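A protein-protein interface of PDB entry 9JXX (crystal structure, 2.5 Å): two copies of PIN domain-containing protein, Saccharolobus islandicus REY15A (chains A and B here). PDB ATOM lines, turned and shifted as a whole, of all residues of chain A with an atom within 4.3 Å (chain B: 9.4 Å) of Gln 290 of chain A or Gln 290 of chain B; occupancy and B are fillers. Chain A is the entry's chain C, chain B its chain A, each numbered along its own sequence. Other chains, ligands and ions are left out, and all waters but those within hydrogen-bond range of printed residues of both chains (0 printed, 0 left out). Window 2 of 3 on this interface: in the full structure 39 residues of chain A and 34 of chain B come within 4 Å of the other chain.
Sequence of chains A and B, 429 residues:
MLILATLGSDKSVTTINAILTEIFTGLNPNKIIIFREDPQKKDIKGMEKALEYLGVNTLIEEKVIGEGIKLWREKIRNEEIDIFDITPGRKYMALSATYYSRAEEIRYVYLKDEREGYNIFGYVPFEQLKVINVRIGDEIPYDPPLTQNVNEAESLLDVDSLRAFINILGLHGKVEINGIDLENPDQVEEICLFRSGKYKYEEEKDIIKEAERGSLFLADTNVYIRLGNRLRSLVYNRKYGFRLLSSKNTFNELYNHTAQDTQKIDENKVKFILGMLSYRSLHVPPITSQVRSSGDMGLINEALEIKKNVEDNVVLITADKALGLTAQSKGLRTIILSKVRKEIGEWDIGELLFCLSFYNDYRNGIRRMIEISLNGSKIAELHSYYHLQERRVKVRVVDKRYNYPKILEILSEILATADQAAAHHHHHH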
ATOM      1  N   LYS A 248     -28.270  -8.908 -13.624  1.00  0.00           N
ATOM      2  CA  LYS A 248     -28.090  -9.534 -12.319  1.00  0.00           C
ATOM      3  C   LYS A 248     -29.418 -10.032 -11.762  1.00  0.00           C
ATOM      4  O   LYS A 248     -29.486 -11.120 -11.179  1.00  0.00           O
ATOM      5  CB  LYS A 248     -27.441  -8.549 -11.350  1.00  0.00           C
ATOM      6  CG  LYS A 248     -26.076  -8.043 -11.789  1.00  0.00           C
ATOM      7  CD  LYS A 248     -25.837  -6.623 -11.301  1.00  0.00           C
ATOM      8  CE  LYS A 248     -25.185  -6.619  -9.929  1.00  0.00           C
ATOM      9  NZ  LYS A 248     -24.693  -5.267  -9.544  1.00  0.00           N
ATOM     10  N   ASN A 252     -30.464 -13.912 -10.748  1.00  0.00           N
ATOM     11  CA  ASN A 252     -30.856 -14.213  -9.375  1.00  0.00           C
ATOM     12  C   ASN A 252     -32.174 -14.975  -9.335  1.00  0.00           C
ATOM     13  O   ASN A 252     -32.320 -15.938  -8.571  1.00  0.00           O
ATOM     14  CB  ASN A 252     -30.958 -12.923  -8.560  1.00  0.00           C
ATOM     15  CG  ASN A 252     -29.612 -12.445  -8.052  1.00  0.00           C
ATOM     16  OD1 ASN A 252     -28.634 -13.194  -8.045  1.00  0.00           O
ATOM     17  ND2 ASN A 252     -29.555 -11.189  -7.622  1.00  0.00           N
ATOM     18  N   ILE A 287     -23.241 -12.438 -11.575  1.00  0.00           N
ATOM     19  CA  ILE A 287     -23.237 -12.464 -10.121  1.00  0.00           C
ATOM     20  C   ILE A 287     -22.036 -13.280  -9.668  1.00  0.00           C
ATOM     21  O   ILE A 287     -22.101 -14.511  -9.572  1.00  0.00           O
ATOM     22  CB  ILE A 287     -24.559 -13.034  -9.570  1.00  0.00           C
ATOM     23  CG1 ILE A 287     -25.698 -12.046  -9.810  1.00  0.00           C
ATOM     24  CG2 ILE A 287     -24.452 -13.325  -8.084  1.00  0.00           C
ATOM     25  CD1 ILE A 287     -25.403 -10.657  -9.302  1.00  0.00           C
ATOM     26  N   SER A 289     -20.943 -12.500  -6.693  1.00  0.00           N
ATOM     27  CA  SER A 289     -21.572 -12.690  -5.386  1.00  0.00           C
ATOM     28  C   SER A 289     -22.668 -11.644  -5.221  1.00  0.00           C
ATOM     29  O   SER A 289     -22.368 -10.451  -5.121  1.00  0.00           O
ATOM     30  CB  SER A 289     -20.541 -12.585  -4.267  1.00  0.00           C
ATOM     31  OG  SER A 289     -20.110 -11.247  -4.092  1.00  0.00           O
ATOM     32  N   GLN A 290     -23.925 -12.092  -5.194  1.00  0.00           N
ATOM     33  CA  GLN A 290     -25.069 -11.288  -4.776  1.00  0.00           C
ATOM     34  C   GLN A 290     -26.293 -12.188  -4.689  1.00  0.00           C
ATOM     35  O   GLN A 290     -26.485 -13.062  -5.538  1.00  0.00           O
ATOM     36  CB  GLN A 290     -25.343 -10.123  -5.740  1.00  0.00           C
ATOM     37  CG  GLN A 290     -26.232  -9.033  -5.156  1.00  0.00           C
ATOM     38  CD  GLN A 290     -26.594  -7.965  -6.168  1.00  0.00           C
ATOM     39  OE1 GLN A 290     -27.456  -8.169  -7.023  1.00  0.00           O
ATOM     40  NE2 GLN A 290     -25.937  -6.814  -6.075  1.00  0.00           N
ATOM     41  N   VAL A 291     -27.117 -11.968  -3.665  1.00  0.00           N
ATOM     42  CA  VAL A 291     -28.361 -12.716  -3.511  1.00  0.00           C
ATOM     43  C   VAL A 291     -29.455 -11.781  -3.011  1.00  0.00           C
ATOM     44  O   VAL A 291     -29.511 -11.448  -1.821  1.00  0.00           O
ATOM     45  CB  VAL A 291     -28.180 -13.920  -2.568  1.00  0.00           C
ATOM     46  CG1 VAL A 291     -27.870 -15.180  -3.368  1.00  0.00           C
ATOM     47  CG2 VAL A 291     -27.078 -13.644  -1.560  1.00  0.00           C
ATOM     48  N   ARG A 292     -30.335 -11.356  -3.916  1.00  0.00           N
ATOM     49  CA  ARG A 292     -31.408 -10.424  -3.581  1.00  0.00           C
ATOM     50  C   ARG A 292     -32.559 -10.663  -4.545  1.00  0.00           C
ATOM     51  O   ARG A 292     -32.383 -10.534  -5.761  1.00  0.00           O
ATOM     52  CB  ARG A 292     -30.912  -8.976  -3.653  1.00  0.00           C
ATOM     53  CG  ARG A 292     -32.002  -7.919  -3.652  1.00  0.00           C
ATOM     54  CD  ARG A 292     -32.074  -7.209  -4.995  1.00  0.00           C
ATOM     55  NE  ARG A 292     -33.022  -6.101  -4.979  1.00  0.00           N
ATOM     56  CZ  ARG A 292     -33.227  -5.275  -5.997  1.00  0.00           C
ATOM     57  NH1 ARG A 292     -32.574  -5.410  -7.139  1.00  0.00           N
ATOM     58  NH2 ARG A 292     -34.117  -4.296  -5.868  1.00  0.00           N
ATOM     59  N   LYS B 248     -13.552  -7.845 -16.306  1.00  0.00           N
ATOM     60  CA  LYS B 248     -13.832  -6.633 -15.543  1.00  0.00           C
ATOM     61  C   LYS B 248     -12.555  -6.055 -14.945  1.00  0.00           C
ATOM     62  O   LYS B 248     -12.403  -4.831 -14.862  1.00  0.00           O
ATOM     63  CB  LYS B 248     -14.857  -6.925 -14.447  1.00  0.00           C
ATOM     64  CG  LYS B 248     -15.486  -5.683 -13.827  1.00  0.00           C
ATOM     65  CD  LYS B 248     -15.958  -4.701 -14.891  1.00  0.00           C
ATOM     66  CE  LYS B 248     -16.370  -3.372 -14.274  1.00  0.00           C
ATOM     67  NZ  LYS B 248     -17.845  -3.264 -14.100  1.00  0.00           N
ATOM     68  N   ASN B 249     -11.632  -6.920 -14.514  1.00  0.00           N
ATOM     69  CA  ASN B 249     -10.363  -6.446 -13.969  1.00  0.00           C
ATOM     70  C   ASN B 249      -9.569  -5.671 -15.011  1.00  0.00           C
ATOM     71  O   ASN B 249      -8.993  -4.619 -14.709  1.00  0.00           O
ATOM     72  CB  ASN B 249      -9.546  -7.629 -13.448  1.00  0.00           C
ATOM     73  CG  ASN B 249      -8.468  -7.211 -12.469  1.00  0.00           C
ATOM     74  OD1 ASN B 249      -8.722  -7.061 -11.276  1.00  0.00           O
ATOM     75  ND2 ASN B 249      -7.253  -7.021 -12.971  1.00  0.00           N
ATOM     76  N   ASN B 252     -11.257  -2.277 -15.691  1.00  0.00           N
ATOM     77  CA  ASN B 252     -11.019  -1.342 -14.597  1.00  0.00           C
ATOM     78  C   ASN B 252      -9.638  -0.709 -14.702  1.00  0.00           C
ATOM     79  O   ASN B 252      -9.484   0.502 -14.509  1.00  0.00           O
ATOM     80  CB  ASN B 252     -11.180  -2.056 -13.254  1.00  0.00           C
ATOM     81  CG  ASN B 252     -12.614  -2.453 -12.972  1.00  0.00           C
ATOM     82  OD1 ASN B 252     -13.532  -2.051 -13.687  1.00  0.00           O
ATOM     83  ND2 ASN B 252     -12.816  -3.255 -11.933  1.00  0.00           N
ATOM     84  N   PRO B 286     -18.134  -4.888 -19.728  1.00  0.00           N
ATOM     85  CA  PRO B 286     -18.916  -5.653 -18.731  1.00  0.00           C
ATOM     86  C   PRO B 286     -19.484  -4.744 -17.641  1.00  0.00           C
ATOM     87  O   PRO B 286     -19.006  -4.669 -16.511  1.00  0.00           O
ATOM     88  CB  PRO B 286     -17.887  -6.643 -18.188  1.00  0.00           C
ATOM     89  CG  PRO B 286     -16.584  -5.921 -18.303  1.00  0.00           C
ATOM     90  CD  PRO B 286     -16.680  -5.026 -19.517  1.00  0.00           C
ATOM     91  N   ILE B 287     -20.548  -4.022 -18.006  1.00  0.00           N
ATOM     92  CA  ILE B 287     -21.120  -3.027 -17.104  1.00  0.00           C
ATOM     93  C   ILE B 287     -21.729  -3.695 -15.877  1.00  0.00           C
ATOM     94  O   ILE B 287     -21.662  -3.157 -14.765  1.00  0.00           O
ATOM     95  CB  ILE B 287     -22.155  -2.165 -17.844  1.00  0.00           C
ATOM     96  CG1 ILE B 287     -21.687  -1.844 -19.263  1.00  0.00           C
ATOM     97  CG2 ILE B 287     -22.401  -0.876 -17.081  1.00  0.00           C
ATOM     98  CD1 ILE B 287     -20.433  -1.005 -19.313  1.00  0.00           C
ATOM     99  N   THR B 288     -22.331  -4.872 -16.055  1.00  0.00           N
ATOM    100  CA  THR B 288     -23.080  -5.514 -14.982  1.00  0.00           C
ATOM    101  C   THR B 288     -22.198  -6.231 -13.966  1.00  0.00           C
ATOM    102  O   THR B 288     -22.688  -6.568 -12.881  1.00  0.00           O
ATOM    103  CB  THR B 288     -24.089  -6.509 -15.564  1.00  0.00           C
ATOM    104  OG1 THR B 288     -23.406  -7.458 -16.393  1.00  0.00           O
ATOM    105  CG2 THR B 288     -25.137  -5.780 -16.395  1.00  0.00           C
ATOM    106  N   SER B 289     -20.928  -6.477 -14.280  1.00  0.00           N
ATOM    107  CA  SER B 289     -20.059  -7.196 -13.358  1.00  0.00           C
ATOM    108  C   SER B 289     -19.756  -6.347 -12.128  1.00  0.00           C
ATOM    109  O   SER B 289     -19.546  -5.135 -12.225  1.00  0.00           O
ATOM    110  CB  SER B 289     -18.759  -7.596 -14.054  1.00  0.00           C
ATOM    111  OG  SER B 289     -17.802  -8.060 -13.116  1.00  0.00           O
ATOM    112  N   GLN B 290     -19.731  -6.997 -10.965  1.00  0.00           N
ATOM    113  CA  GLN B 290     -19.474  -6.325  -9.698  1.00  0.00           C
ATOM    114  C   GLN B 290     -18.006  -6.354  -9.291  1.00  0.00           C
ATOM    115  O   GLN B 290     -17.672  -5.873  -8.203  1.00  0.00           O
ATOM    116  CB  GLN B 290     -20.326  -6.951  -8.588  1.00  0.00           C
ATOM    117  CG  GLN B 290     -21.747  -7.281  -9.009  1.00  0.00           C
ATOM    118  CD  GLN B 290     -22.639  -7.623  -7.830  1.00  0.00           C
ATOM    119  OE1 GLN B 290     -23.136  -8.743  -7.718  1.00  0.00           O
ATOM    120  NE2 GLN B 290     -22.849  -6.654  -6.947  1.00  0.00           N
ATOM    121  N   VAL B 291     -17.128  -6.910 -10.127  1.00  0.00           N
ATOM    122  CA  VAL B 291     -15.704  -6.952  -9.812  1.00  0.00           C
ATOM    123  C   VAL B 291     -15.152  -5.533  -9.789  1.00  0.00           C
ATOM    124  O   VAL B 291     -15.414  -4.732 -10.699  1.00  0.00           O
ATOM    125  CB  VAL B 291     -14.958  -7.833 -10.825  1.00  0.00           C
ATOM    126  CG1 VAL B 291     -13.455  -7.605 -10.738  1.00  0.00           C
ATOM    127  CG2 VAL B 291     -15.295  -9.300 -10.600  1.00  0.00           C
ATOM    128  N   ARG B 292     -14.386  -5.208  -8.744  1.00  0.00           N
ATOM    129  CA  ARG B 292     -13.902  -3.848  -8.527  1.00  0.00           C
ATOM    130  C   ARG B 292     -12.380  -3.776  -8.422  1.00  0.00           C
ATOM    131  O   ARG B 292     -11.845  -2.761  -7.965  1.00  0.00           O
ATOM    132  CB  ARG B 292     -14.548  -3.254  -7.273  1.00  0.00           C
ATOM    133  CG  ARG B 292     -15.896  -2.594  -7.521  1.00  0.00           C
ATOM    134  CD  ARG B 292     -16.687  -2.438  -6.229  1.00  0.00           C
ATOM    135  NE  ARG B 292     -18.114  -2.659  -6.431  1.00  0.00           N
ATOM    136  CZ  ARG B 292     -18.955  -3.057  -5.485  1.00  0.00           C
ATOM    137  NH1 ARG B 292     -18.543  -3.291  -4.250  1.00  0.00           N
ATOM    138  NH2 ARG B 292     -20.238  -3.227  -5.788  1.00  0.00           N
ATOM    139  N   SER B 293     -11.672  -4.820  -8.836  1.00  0.00           N
ATOM    140  CA  SER B 293     -10.220  -4.851  -8.755  1.00  0.00           C
ATOM    141  C   SER B 293      -9.595  -4.449 -10.087  1.00  0.00           C
ATOM    142  O   SER B 293     -10.221  -4.534 -11.146  1.00  0.00           O
ATOM    143  CB  SER B 293      -9.732  -6.242  -8.346  1.00  0.00           C
ATOM    144  OG  SER B 293     -10.336  -7.239  -9.152  1.00  0.00           O
ATOM    145  N   GLU B 302     -10.587 -13.142 -10.601  1.00  0.00           N
ATOM    146  CA  GLU B 302     -11.738 -13.064 -11.495  1.00  0.00           C
ATOM    147  C   GLU B 302     -11.827 -14.306 -12.372  1.00  0.00           C
ATOM    148  O   GLU B 302     -12.915 -14.862 -12.568  1.00  0.00           O
ATOM    149  CB  GLU B 302     -11.665 -11.808 -12.366  1.00  0.00           C
ATOM    150  CG  GLU B 302     -12.742 -11.764 -13.446  1.00  0.00           C
ATOM    151  CD  GLU B 302     -12.713 -10.495 -14.277  1.00  0.00           C
ATOM    152  OE1 GLU B 302     -11.664  -9.820 -14.308  1.00  0.00           O
ATOM    153  OE2 GLU B 302     -13.745 -10.172 -14.904  1.00  0.00           O
ATOM    154  N   GLU B 305     -13.105 -17.247 -10.266  1.00  0.00           N
ATOM    155  CA  GLU B 305     -14.537 -17.180  -9.987  1.00  0.00           C
ATOM    156  C   GLU B 305     -15.355 -17.598 -11.202  1.00  0.00           C
ATOM    157  O   GLU B 305     -16.349 -18.323 -11.071  1.00  0.00           O
ATOM    158  CB  GLU B 305     -14.921 -15.771  -9.541  1.00  0.00           C
ATOM    159  CG  GLU B 305     -15.027 -15.597  -8.031  1.00  0.00           C
ATOM    160  CD  GLU B 305     -15.742 -16.751  -7.355  1.00  0.00           C
ATOM    161  OE1 GLU B 305     -15.058 -17.619  -6.771  1.00  0.00           O
ATOM    162  OE2 GLU B 305     -16.990 -16.791  -7.405  1.00  0.00           O
ATOM    163  N   ASN B 309     -17.820 -21.405 -11.912  1.00  0.00           N
ATOM    164  CA  ASN B 309     -19.256 -21.308 -12.132  1.00  0.00           C
ATOM    165  C   ASN B 309     -19.702 -21.517 -13.573  1.00  0.00           C
ATOM    166  O   ASN B 309     -20.899 -21.375 -13.853  1.00  0.00           O
ATOM    167  CB  ASN B 309     -19.763 -19.944 -11.644  1.00  0.00           C
ATOM    168  CG  ASN B 309     -19.591 -19.759 -10.147  1.00  0.00           C
ATOM    169  OD1 ASN B 309     -19.896 -20.655  -9.359  1.00  0.00           O
ATOM    170  ND2 ASN B 309     -19.091 -18.595  -9.749  1.00  0.00           N
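The side-chain amide nitrogen (NE2) of Gln 290 of chain B sits close to the side-chain amino group (NZ) of Lys 248 of chain A (3.5 Å). OE1 of Gln 290 of chain B lies close to O of Ser 289 of chain A (3.2 Å). The side-chain amide nitrogen of Gln 290 of chain B sits close to the side-chain amide nitrogen of Gln 290 of chain A, 3.2 Å away.
OD1 of Asn 252 of chain A lies close to O of Gln 290 of chain A.
Lys 248 of chain A touches Thr 288 of chain B. Gln 290 of chain B touches Ile 287 of chain A (OE1 to CD1, 3.4 Å).
Printed residues of chain B within 4 Å of Gln 290 of chain A: Gln 290 (3.2 Å). Of chain B, only Gln 290 (3.4 Å) comes within 4 Å of Ile 287 of chain A. Of chain B, only Gln 290 (3.2 Å) comes within 4 Å of Ser 289 of chain A. No residue of chain B comes within 4 Å of Val 291 of chain A. Printed residues of chain A within 4 Å of Thr 288 of chain B: Lys 248 (3.5 Å). Of the printed residues of chain B, Lys 248 of chain A touches Thr 288 and Gln 290. Arg 292 of chain B touches none of the printed residues of chain A. The nearest residue of chain B that does not touch Gln 290 of chain A is Arg 292 of chain B (6.7 Å).
Of the 7 printed residues of chain A, 4 touch a printed residue of chain B. Of the 14 printed residues of chain B, 2 touch a printed residue of chain A. Among the printed residues, 5 pairs touch across the chains. Among the printed residues, no Asp or Glu carboxylate lies within 4 Å of a Lys or Arg side-chain nitrogen of the other chain.
Lys 248 of chain A touches Gln 290 of chain B, but with the chains exchanged Gln 290 of chain A does not touch Lys 248 of chain B (11.9 Å). Ile 287 of chain A touches Gln 290 of chain B, but with the chains exchanged Gln 290 of chain A does not touch Ile 287 of chain B (10.4 Å). Ser 289 of chain A touches Gln 290 of chain B, but with the chains exchanged Gln 290 of chain A does not touch Ser 289 of chain B (8.7 Å). Gln 290 of chain A touches its own counterpart, Gln 290 of chain B. Of the 5 pairs that touch across the chains among the printed residues, 1 has its exchanged pair printed and touching as well.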
